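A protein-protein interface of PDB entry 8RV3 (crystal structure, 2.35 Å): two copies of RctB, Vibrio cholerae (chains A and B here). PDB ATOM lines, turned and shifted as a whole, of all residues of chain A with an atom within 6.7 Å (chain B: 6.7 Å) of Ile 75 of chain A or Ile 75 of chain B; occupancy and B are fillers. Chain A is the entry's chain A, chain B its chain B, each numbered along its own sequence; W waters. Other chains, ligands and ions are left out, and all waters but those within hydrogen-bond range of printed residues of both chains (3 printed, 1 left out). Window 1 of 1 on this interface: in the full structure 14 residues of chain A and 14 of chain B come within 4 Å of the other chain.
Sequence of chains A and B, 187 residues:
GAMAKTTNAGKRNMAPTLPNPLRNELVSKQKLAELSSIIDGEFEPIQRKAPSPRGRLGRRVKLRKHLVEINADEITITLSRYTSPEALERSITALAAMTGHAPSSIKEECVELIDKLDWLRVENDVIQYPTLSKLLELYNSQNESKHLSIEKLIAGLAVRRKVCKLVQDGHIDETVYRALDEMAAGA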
ATOM      1  N   ILE A  70      13.585 -27.101 -26.272  1.00  0.00           N
ATOM      2  CA  ILE A  70      12.828 -28.197 -25.606  1.00  0.00           C
ATOM      3  C   ILE A  70      11.508 -27.654 -25.066  1.00  0.00           C
ATOM      4  O   ILE A  70      11.497 -26.775 -24.222  1.00  0.00           O
ATOM      5  CB  ILE A  70      13.612 -28.931 -24.547  1.00  0.00           C
ATOM      6  CG1 ILE A  70      14.950 -29.447 -25.168  1.00  0.00           C
ATOM      7  CG2 ILE A  70      12.718 -30.090 -24.061  1.00  0.00           C
ATOM      8  CD1 ILE A  70      16.152 -29.337 -24.408  1.00  0.00           C
ATOM      9  N   ASN A  71      10.404 -28.122 -25.652  1.00  0.00           N
ATOM     10  CA  ASN A  71       9.035 -27.672 -25.463  1.00  0.00           C
ATOM     11  C   ASN A  71       8.263 -28.676 -24.604  1.00  0.00           C
ATOM     12  O   ASN A  71       8.164 -29.848 -25.002  1.00  0.00           O
ATOM     13  CB  ASN A  71       8.381 -27.536 -26.883  1.00  0.00           C
ATOM     14  CG  ASN A  71       9.170 -26.541 -27.726  1.00  0.00           C
ATOM     15  OD1 ASN A  71       9.412 -25.430 -27.201  1.00  0.00           O
ATOM     16  ND2 ASN A  71       9.642 -26.889 -29.013  1.00  0.00           N
ATOM     17  N   ALA A  72       7.701 -28.244 -23.468  1.00  0.00           N
ATOM     18  CA  ALA A  72       6.891 -29.113 -22.612  1.00  0.00           C
ATOM     19  C   ALA A  72       5.736 -28.342 -22.067  1.00  0.00           C
ATOM     20  O   ALA A  72       5.845 -27.711 -21.022  1.00  0.00           O
ATOM     21  CB  ALA A  72       7.712 -29.628 -21.455  1.00  0.00           C
ATOM     22  N   ASP A  73       4.631 -28.355 -22.813  1.00  0.00           N
ATOM     23  CA  ASP A  73       3.407 -27.622 -22.573  1.00  0.00           C
ATOM     24  C   ASP A  73       3.687 -26.093 -22.467  1.00  0.00           C
ATOM     25  O   ASP A  73       4.056 -25.481 -23.490  1.00  0.00           O
ATOM     26  CB  ASP A  73       2.589 -28.182 -21.445  1.00  0.00           C
ATOM     27  CG  ASP A  73       2.165 -29.626 -21.533  1.00  0.00           C
ATOM     28  OD1 ASP A  73       1.693 -30.045 -22.571  1.00  0.00           O
ATOM     29  OD2 ASP A  73       2.246 -30.322 -20.518  1.00  0.00           O
ATOM     30  N   GLU A  74       3.522 -25.482 -21.276  1.00  0.00           N
ATOM     31  CA  GLU A  74       3.697 -24.034 -21.072  1.00  0.00           C
ATOM     32  C   GLU A  74       5.114 -23.564 -21.199  1.00  0.00           C
ATOM     33  O   GLU A  74       5.339 -22.374 -21.346  1.00  0.00           O
ATOM     34  CB  GLU A  74       3.149 -23.624 -19.657  1.00  0.00           C
ATOM     35  CG  GLU A  74       1.638 -23.665 -19.604  1.00  0.00           C
ATOM     36  CD  GLU A  74       1.055 -25.053 -19.502  1.00  0.00           C
ATOM     37  OE1 GLU A  74       1.775 -25.944 -19.011  1.00  0.00           O
ATOM     38  OE2 GLU A  74      -0.119 -25.256 -19.879  1.00  0.00           O
ATOM     39  N   ILE A  75       6.066 -24.464 -21.034  1.00  0.00           N
ATOM     40  CA  ILE A  75       7.490 -24.123 -21.090  1.00  0.00           C
ATOM     41  C   ILE A  75       8.227 -24.380 -22.445  1.00  0.00           C
ATOM     42  O   ILE A  75       8.036 -25.389 -23.127  1.00  0.00           O
ATOM     43  CB  ILE A  75       8.156 -24.937 -19.954  1.00  0.00           C
ATOM     44  CG1 ILE A  75       9.459 -24.350 -19.504  1.00  0.00           C
ATOM     45  CG2 ILE A  75       8.411 -26.371 -20.393  1.00  0.00           C
ATOM     46  CD1 ILE A  75      10.093 -25.143 -18.189  1.00  0.00           C
ATOM     47  N   THR A  76       9.174 -23.514 -22.723  1.00  0.00           N
ATOM     48  CA  THR A  76      10.165 -23.719 -23.740  1.00  0.00           C
ATOM     49  C   THR A  76      11.558 -23.463 -23.071  1.00  0.00           C
ATOM     50  O   THR A  76      11.756 -22.429 -22.454  1.00  0.00           O
ATOM     51  CB  THR A  76       9.990 -22.898 -25.032  1.00  0.00           C
ATOM     52  OG1 THR A  76       8.885 -23.423 -25.798  1.00  0.00           O
ATOM     53  CG2 THR A  76      11.240 -23.072 -25.973  1.00  0.00           C
ATOM     54  N   ILE A  77      12.478 -24.400 -23.139  1.00  0.00           N
ATOM     55  CA  ILE A  77      13.869 -24.214 -22.651  1.00  0.00           C
ATOM     56  C   ILE A  77      14.771 -24.147 -23.907  1.00  0.00           C
ATOM     57  O   ILE A  77      14.640 -24.979 -24.814  1.00  0.00           O
ATOM     58  CB  ILE A  77      14.352 -25.366 -21.700  1.00  0.00           C
ATOM     59  CG1 ILE A  77      13.478 -25.486 -20.392  1.00  0.00           C
ATOM     60  CG2 ILE A  77      15.813 -25.214 -21.369  1.00  0.00           C
ATOM     61  CD1 ILE A  77      13.756 -24.384 -19.329  1.00  0.00           C
ATOM     62  N   THR A  78      15.643 -23.114 -24.001  1.00  0.00           N
ATOM     63  CA  THR A  78      16.548 -23.001 -25.117  1.00  0.00           C
ATOM     64  C   THR A  78      17.985 -23.103 -24.617  1.00  0.00           C
ATOM     65  O   THR A  78      18.366 -22.349 -23.710  1.00  0.00           O
ATOM     66  CB  THR A  78      16.259 -21.741 -25.931  1.00  0.00           C
ATOM     67  OG1 THR A  78      14.942 -21.849 -26.388  1.00  0.00           O
ATOM     68  CG2 THR A  78      17.218 -21.560 -27.105  1.00  0.00           C
ATOM     69  N   SER A  91      17.707 -25.555 -15.605  1.00  0.00           N
ATOM     70  CA  SER A  91      16.888 -25.918 -16.785  1.00  0.00           C
ATOM     71  C   SER A  91      16.347 -27.343 -16.650  1.00  0.00           C
ATOM     72  O   SER A  91      15.166 -27.563 -16.816  1.00  0.00           O
ATOM     73  CB  SER A  91      17.683 -25.775 -18.086  1.00  0.00           C
ATOM     74  OG  SER A  91      17.907 -24.402 -18.323  1.00  0.00           O
ATOM     75  N   ALA A  94      13.549 -27.097 -13.897  1.00  0.00           N
ATOM     76  CA  ALA A  94      12.404 -26.530 -14.591  1.00  0.00           C
ATOM     77  C   ALA A  94      11.710 -27.590 -15.575  1.00  0.00           C
ATOM     78  O   ALA A  94      10.529 -27.768 -15.478  1.00  0.00           O
ATOM     79  CB  ALA A  94      12.809 -25.256 -15.336  1.00  0.00           C
ATOM     80  N   LEU A  95      12.425 -28.338 -16.389  1.00  0.00           N
ATOM     81  CA  LEU A  95      11.786 -29.403 -17.210  1.00  0.00           C
ATOM     82  C   LEU A  95      11.227 -30.508 -16.329  1.00  0.00           C
ATOM     83  O   LEU A  95      10.168 -30.975 -16.637  1.00  0.00           O
ATOM     84  CB  LEU A  95      12.717 -30.068 -18.239  1.00  0.00           C
ATOM     85  CG  LEU A  95      13.130 -29.235 -19.371  1.00  0.00           C
ATOM     86  CD1 LEU A  95      14.426 -29.879 -20.095  1.00  0.00           C
ATOM     87  CD2 LEU A  95      11.946 -28.868 -20.219  1.00  0.00           C
ATOM     88  N   MET A  98       7.775 -29.762 -15.069  1.00  0.00           N
ATOM     89  CA  MET A  98       6.701 -29.772 -16.069  1.00  0.00           C
ATOM     90  C   MET A  98       6.326 -31.196 -16.504  1.00  0.00           C
ATOM     91  O   MET A  98       5.178 -31.503 -16.810  1.00  0.00           O
ATOM     92  CB  MET A  98       7.123 -28.977 -17.344  1.00  0.00           C
ATOM     93  CG  MET A  98       7.490 -27.534 -17.091  1.00  0.00           C
ATOM     94  SD  MET A  98       6.182 -26.587 -16.272  1.00  0.00           S
ATOM     95  CE  MET A  98       4.793 -26.785 -17.449  1.00  0.00           C
ATOM     96  N   THR A  99       7.344 -32.040 -16.658  1.00  0.00           N
ATOM     97  CA  THR A  99       7.202 -33.345 -17.263  1.00  0.00           C
ATOM     98  C   THR A  99       7.063 -34.458 -16.271  1.00  0.00           C
ATOM     99  O   THR A  99       6.468 -35.475 -16.622  1.00  0.00           O
ATOM    100  CB  THR A  99       8.391 -33.594 -18.251  1.00  0.00           C
ATOM    101  OG1 THR A  99       9.587 -33.697 -17.512  1.00  0.00           O
ATOM    102  CG2 THR A  99       8.534 -32.465 -19.304  1.00  0.00           C
ATOM    103  N   GLU A 151      19.730 -15.692 -27.046  1.00  0.00           N
ATOM    104  CA  GLU A 151      19.162 -16.622 -28.013  1.00  0.00           C
ATOM    105  C   GLU A 151      18.935 -15.929 -29.345  1.00  0.00           C
ATOM    106  O   GLU A 151      19.225 -16.521 -30.352  1.00  0.00           O
ATOM    107  CB  GLU A 151      17.849 -17.259 -27.484  1.00  0.00           C
ATOM    108  CG  GLU A 151      18.098 -18.139 -26.247  1.00  0.00           C
ATOM    109  CD  GLU A 151      18.170 -17.437 -24.889  1.00  0.00           C
ATOM    110  OE1 GLU A 151      17.789 -16.245 -24.854  1.00  0.00           O
ATOM    111  OE2 GLU A 151      18.586 -18.056 -23.868  1.00  0.00           O
ATOM    112  N   ILE B  70       6.404 -15.013 -20.245  1.00  0.00           N
ATOM    113  CA  ILE B  70       7.370 -14.692 -19.158  1.00  0.00           C
ATOM    114  C   ILE B  70       8.712 -15.352 -19.481  1.00  0.00           C
ATOM    115  O   ILE B  70       8.817 -16.582 -19.584  1.00  0.00           O
ATOM    116  CB  ILE B  70       6.879 -15.135 -17.791  1.00  0.00           C
ATOM    117  CG1 ILE B  70       5.594 -14.408 -17.526  1.00  0.00           C
ATOM    118  CG2 ILE B  70       7.935 -14.794 -16.685  1.00  0.00           C
ATOM    119  CD1 ILE B  70       4.518 -15.196 -16.776  1.00  0.00           C
ATOM    120  N   ASN B  71       9.722 -14.507 -19.676  1.00  0.00           N
ATOM    121  CA  ASN B  71      11.046 -14.843 -20.118  1.00  0.00           C
ATOM    122  C   ASN B  71      12.055 -14.718 -18.980  1.00  0.00           C
ATOM    123  O   ASN B  71      12.190 -13.615 -18.429  1.00  0.00           O
ATOM    124  CB  ASN B  71      11.352 -13.854 -21.207  1.00  0.00           C
ATOM    125  CG  ASN B  71      10.384 -13.999 -22.417  1.00  0.00           C
ATOM    126  OD1 ASN B  71      10.173 -15.138 -22.874  1.00  0.00           O
ATOM    127  ND2 ASN B  71       9.754 -12.898 -22.975  1.00  0.00           N
ATOM    128  N   ALA B  72      12.768 -15.837 -18.609  1.00  0.00           N
ATOM    129  CA  ALA B  72      13.738 -15.844 -17.501  1.00  0.00           C
ATOM    130  C   ALA B  72      14.899 -16.696 -17.939  1.00  0.00           C
ATOM    131  O   ALA B  72      14.875 -17.938 -17.845  1.00  0.00           O
ATOM    132  CB  ALA B  72      13.116 -16.399 -16.237  1.00  0.00           C
ATOM    133  N   ASP B  73      15.913 -16.026 -18.488  1.00  0.00           N
ATOM    134  CA  ASP B  73      17.081 -16.683 -19.065  1.00  0.00           C
ATOM    135  C   ASP B  73      16.691 -17.775 -20.129  1.00  0.00           C
ATOM    136  O   ASP B  73      16.146 -17.464 -21.166  1.00  0.00           O
ATOM    137  CB  ASP B  73      18.010 -17.219 -17.967  1.00  0.00           C
ATOM    138  CG  ASP B  73      18.591 -16.186 -17.046  1.00  0.00           C
ATOM    139  OD1 ASP B  73      19.095 -15.146 -17.560  1.00  0.00           O
ATOM    140  OD2 ASP B  73      18.637 -16.458 -15.808  1.00  0.00           O
ATOM    141  N   GLU B  74      17.020 -19.066 -19.867  1.00  0.00           N
ATOM    142  CA  GLU B  74      16.747 -20.179 -20.783  1.00  0.00           C
ATOM    143  C   GLU B  74      15.288 -20.496 -20.963  1.00  0.00           C
ATOM    144  O   GLU B  74      14.903 -21.121 -21.966  1.00  0.00           O
ATOM    145  CB  GLU B  74      17.514 -21.447 -20.371  1.00  0.00           C
ATOM    146  CG  GLU B  74      18.987 -21.297 -20.564  1.00  0.00           C
ATOM    147  CD  GLU B  74      19.729 -20.492 -19.524  1.00  0.00           C
ATOM    148  OE1 GLU B  74      19.244 -20.390 -18.393  1.00  0.00           O
ATOM    149  OE2 GLU B  74      20.815 -19.967 -19.829  1.00  0.00           O
ATOM    150  N   ILE B  75      14.454 -20.046 -20.044  1.00  0.00           N
ATOM    151  CA  ILE B  75      13.025 -20.353 -20.084  1.00  0.00           C
ATOM    152  C   ILE B  75      12.107 -19.261 -20.622  1.00  0.00           C
ATOM    153  O   ILE B  75      12.291 -18.052 -20.371  1.00  0.00           O
ATOM    154  CB  ILE B  75      12.630 -20.730 -18.639  1.00  0.00           C
ATOM    155  CG1 ILE B  75      11.391 -21.606 -18.588  1.00  0.00           C
ATOM    156  CG2 ILE B  75      12.423 -19.485 -17.781  1.00  0.00           C
ATOM    157  CD1 ILE B  75      11.032 -22.185 -17.093  1.00  0.00           C
ATOM    158  N   THR B  76      11.047 -19.713 -21.303  1.00  0.00           N
ATOM    159  CA  THR B  76       9.917 -18.882 -21.667  1.00  0.00           C
ATOM    160  C   THR B  76       8.687 -19.658 -21.207  1.00  0.00           C
ATOM    161  O   THR B  76       8.532 -20.835 -21.539  1.00  0.00           O
ATOM    162  CB  THR B  76       9.823 -18.483 -23.171  1.00  0.00           C
ATOM    163  OG1 THR B  76      10.850 -17.514 -23.446  1.00  0.00           O
ATOM    164  CG2 THR B  76       8.461 -17.808 -23.465  1.00  0.00           C
ATOM    165  N   ILE B  77       7.840 -19.044 -20.410  1.00  0.00           N
ATOM    166  CA  ILE B  77       6.576 -19.657 -19.981  1.00  0.00           C
ATOM    167  C   ILE B  77       5.439 -18.867 -20.680  1.00  0.00           C
ATOM    168  O   ILE B  77       5.492 -17.635 -20.734  1.00  0.00           O
ATOM    169  CB  ILE B  77       6.394 -19.650 -18.390  1.00  0.00           C
ATOM    170  CG1 ILE B  77       7.470 -20.467 -17.635  1.00  0.00           C
ATOM    171  CG2 ILE B  77       5.015 -20.147 -18.000  1.00  0.00           C
ATOM    172  CD1 ILE B  77       7.286 -22.043 -17.765  1.00  0.00           C
ATOM    173  N   THR B  78       4.470 -19.553 -21.292  1.00  0.00           N
ATOM    174  CA  THR B  78       3.328 -18.871 -21.923  1.00  0.00           C
ATOM    175  C   THR B  78       2.035 -19.264 -21.224  1.00  0.00           C
ATOM    176  O   THR B  78       1.770 -20.458 -21.103  1.00  0.00           O
ATOM    177  CB  THR B  78       3.301 -19.097 -23.430  1.00  0.00           C
ATOM    178  OG1 THR B  78       4.527 -18.534 -23.878  1.00  0.00           O
ATOM    179  CG2 THR B  78       2.049 -18.421 -24.150  1.00  0.00           C
ATOM    180  N   ARG B  90       2.891 -26.263 -11.859  1.00  0.00           N
ATOM    181  CA  ARG B  90       4.131 -26.675 -12.566  1.00  0.00           C
ATOM    182  C   ARG B  90       4.865 -25.481 -13.161  1.00  0.00           C
ATOM    183  O   ARG B  90       6.063 -25.384 -12.944  1.00  0.00           O
ATOM    184  CB  ARG B  90       3.821 -27.697 -13.656  1.00  0.00           C
ATOM    185  CG  ARG B  90       3.211 -28.929 -13.069  1.00  0.00           C
ATOM    186  CD  ARG B  90       3.040 -30.077 -14.040  1.00  0.00           C
ATOM    187  NE  ARG B  90       2.012 -29.884 -15.060  1.00  0.00           N
ATOM    188  CZ  ARG B  90       0.731 -30.206 -14.891  1.00  0.00           C
ATOM    189  NH1 ARG B  90       0.286 -30.588 -13.700  1.00  0.00           N
ATOM    190  NH2 ARG B  90      -0.138 -30.045 -15.878  1.00  0.00           N
ATOM    191  N   SER B  91       4.175 -24.538 -13.810  1.00  0.00           N
ATOM    192  CA  SER B  91       4.796 -23.332 -14.397  1.00  0.00           C
ATOM    193  C   SER B  91       5.472 -22.442 -13.366  1.00  0.00           C
ATOM    194  O   SER B  91       6.635 -22.114 -13.497  1.00  0.00           O
ATOM    195  CB  SER B  91       3.767 -22.543 -15.237  1.00  0.00           C
ATOM    196  OG  SER B  91       3.400 -23.286 -16.381  1.00  0.00           O
ATOM    197  N   ALA B  94       8.631 -24.323 -12.232  1.00  0.00           N
ATOM    198  CA  ALA B  94       9.617 -24.190 -13.283  1.00  0.00           C
ATOM    199  C   ALA B  94      10.194 -22.722 -13.253  1.00  0.00           C
ATOM    200  O   ALA B  94      11.373 -22.602 -13.311  1.00  0.00           O
ATOM    201  CB  ALA B  94       8.992 -24.547 -14.632  1.00  0.00           C
ATOM    202  N   LEU B  95       9.428 -21.632 -13.119  1.00  0.00           N
ATOM    203  CA  LEU B  95      10.024 -20.263 -12.987  1.00  0.00           C
ATOM    204  C   LEU B  95      10.863 -20.142 -11.722  1.00  0.00           C
ATOM    205  O   LEU B  95      11.897 -19.499 -11.798  1.00  0.00           O
ATOM    206  CB  LEU B  95       9.004 -19.122 -12.947  1.00  0.00           C
ATOM    207  CG  LEU B  95       8.310 -18.834 -14.167  1.00  0.00           C
ATOM    208  CD1 LEU B  95       7.053 -17.981 -13.905  1.00  0.00           C
ATOM    209  CD2 LEU B  95       9.291 -18.310 -15.236  1.00  0.00           C
ATOM    210  N   MET B  98      14.356 -21.456 -12.130  1.00  0.00           N
ATOM    211  CA  MET B  98      15.247 -20.631 -12.965  1.00  0.00           C
ATOM    212  C   MET B  98      15.743 -19.372 -12.247  1.00  0.00           C
ATOM    213  O   MET B  98      16.913 -18.973 -12.391  1.00  0.00           O
ATOM    214  CB  MET B  98      14.540 -20.181 -14.296  1.00  0.00           C
ATOM    215  CG  MET B  98      14.041 -21.342 -15.116  1.00  0.00           C
ATOM    216  SD  MET B  98      15.417 -22.493 -15.514  1.00  0.00           S
ATOM    217  CE  MET B  98      16.534 -21.372 -16.430  1.00  0.00           C
ATOM    218  N   THR B  99      14.842 -18.724 -11.559  1.00  0.00           N
ATOM    219  CA  THR B  99      15.065 -17.416 -10.972  1.00  0.00           C
ATOM    220  C   THR B  99      15.559 -17.479  -9.537  1.00  0.00           C
ATOM    221  O   THR B  99      16.224 -16.560  -9.105  1.00  0.00           O
ATOM    222  CB  THR B  99      13.730 -16.593 -11.093  1.00  0.00           C
ATOM    223  OG1 THR B  99      12.704 -17.202 -10.300  1.00  0.00           O
ATOM    224  CG2 THR B  99      13.182 -16.489 -12.525  1.00  0.00           C
ATOM    225  N   GLU B 151      -1.555 -22.716 -27.434  1.00  0.00           N
ATOM    226  CA  GLU B 151      -1.051 -21.362 -27.614  1.00  0.00           C
ATOM    227  C   GLU B 151      -1.249 -20.874 -29.068  1.00  0.00           C
ATOM    228  O   GLU B 151      -1.571 -19.727 -29.246  1.00  0.00           O
ATOM    229  CB  GLU B 151       0.438 -21.255 -27.174  1.00  0.00           C
ATOM    230  CG  GLU B 151       0.598 -21.520 -25.657  1.00  0.00           C
ATOM    231  CD  GLU B 151       0.861 -22.991 -25.371  1.00  0.00           C
ATOM    232  OE1 GLU B 151       1.062 -23.771 -26.347  1.00  0.00           O
ATOM    233  OE2 GLU B 151       0.880 -23.366 -24.174  1.00  0.00           O
HETATM  234  O   HOH W   1      13.544 -20.602 -24.374  1.00  0.00           O
HETATM  235  O   HOH W   2       0.428 -26.002 -22.899  1.00  0.00           O
HETATM  236  O   HOH W   3       1.663 -28.531 -18.001  1.00  0.00           O
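The backbone carbonyl oxygen of Thr 76 of chain A sits close to the backbone carbonyl oxygen of Glu 74 of chain B (3.4 Å). The side-chain sulfur of Met 98 of chain A sits close to the backbone carbonyl oxygen of Arg 90 of chain B (3.5 Å). The backbone NH of Thr 78 of chain A sits at hydrogen-bond distance from the backbone carbonyl oxygen of Glu 74 of chain B. The side-chain sulfur (SD) of Met 98 of chain A is in hydrogen-bond range of the backbone NH (N) of Ser 91 of chain B, 3.8 Å away. O of Thr 76 of chain B lies within hydrogen-bond range of N of Thr 76 of chain A, at 3.0 Å. N of Thr 78 of chain B is in hydrogen-bond range of O of Glu 74 of chain A (3.0 Å).
The side-chain amide oxygen (OD1) of Asn 71 of chain A is in hydrogen-bond range of the side-chain hydroxyl (OG1) of Thr 76 of chain A (2.5 Å). O of Ile 77 of chain A sits at hydrogen-bond distance from N of Ile 70 of chain A. The side-chain amide oxygen (OD1) of Asn 71 of chain B sits at hydrogen-bond distance from the side-chain hydroxyl (OG1) of Thr 76 of chain B (2.5 Å). The backbone carbonyl oxygen (O) of Ile 70 of chain B sits at hydrogen-bond distance from the backbone NH (N) of Ile 77 of chain B (2.8 Å).
OE2 of Glu 151 of chain B touches O of Asp 73 of chain A, 3.9 Å away. Glu 74 of chain A touches Thr 76 of chain B (O to O, 3.5 Å). CA of Ile 77 of chain B touches O of Glu 74 of chain A (3.3 Å). Glu 74 of chain A touches Ser 91 of chain B (CB to OG, 3.3 Å). CD1 of Ile 75 of chain B touches CD1 of Ile 75 of chain A, 3.3 Å away. Thr 76 of chain A touches Ile 75 of chain B (O to CA, 3.4 Å). CA of Ile 77 of chain A touches O of Glu 74 of chain B, 3.3 Å away. SD of Met 98 of chain B touches N of Ser 91 of chain A, 3.8 Å away. Ile 75 of chain B touches Ala 94 of chain A. OE2 of Glu 151 of chain A touches O of Asp 73 of chain B, at 3.7 Å.
Of the printed residues of chain B, Glu 74 of chain A touches Thr 76, Ile 77, Thr 78 and Ser 91. Ile 75 of chain A touches four residues of chain B. Of the printed residues of chain A, Glu 74 of chain B touches Thr 76, Ile 77, Thr 78 and Ser 91. The nearest printed residue of chain A that does not touch Arg 90 of chain B is Asp 73 of chain A (5.2 Å).
Hydrophobic or aromatic side chains of chain B that line the printed part of chain A: Ile 75, Ile 77, Ala 94 and Met 98. Along chain B the printed residues that touch a printed residue of chain A span positions 73 to 151. Of the 15 printed residues of chain A, 10 touch a printed residue of chain B. Hydrophobic or aromatic side chains of chain A within 4 Å of the printed part of chain B: Ile 75, Ile 77, Ala 94 and Met 98. Among the printed residues, 24 pairs touch across the chains.
Glu 74 of chain A touches Thr 76 of chain B, and with the chains exchanged Thr 76 of chain A touches Glu 74 of chain B. Glu 74 of chain A touches Thr 78 of chain B, and with the chains exchanged Thr 78 of chain A touches Glu 74 of chain B. Ile 75 of chain B touches its own counterpart, Ile 75 of chain A. Ile 75 of chain A touches Ala 94 of chain B, and with the chains exchanged Ala 94 of chain A touches Ile 75 of chain B. 15 positions are printed for both chains. Of the 24 pairs that touch across the chains among the printed residues, 23 have their exchanged pair printed and touching as well.
Water W1 lies within hydrogen-bond range of OG1 of Thr 78 of chain A (2.8 Å), O of Glu 74 of chain B (2.8 Å) and O of Thr 76 of chain A (3.2 Å). Water W3 lies within hydrogen-bond range of OE1 of Glu 74 of chain A (2.8 Å), OD2 of Asp 73 of chain A (3.1 Å) and NH2 of Arg 90 of chain B (3.2 Å). Water W2 lies within hydrogen-bond range of OE2 of Glu 151 of chain B (3.0 Å) and OE2 of Glu 74 of chain A (3.2 Å).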
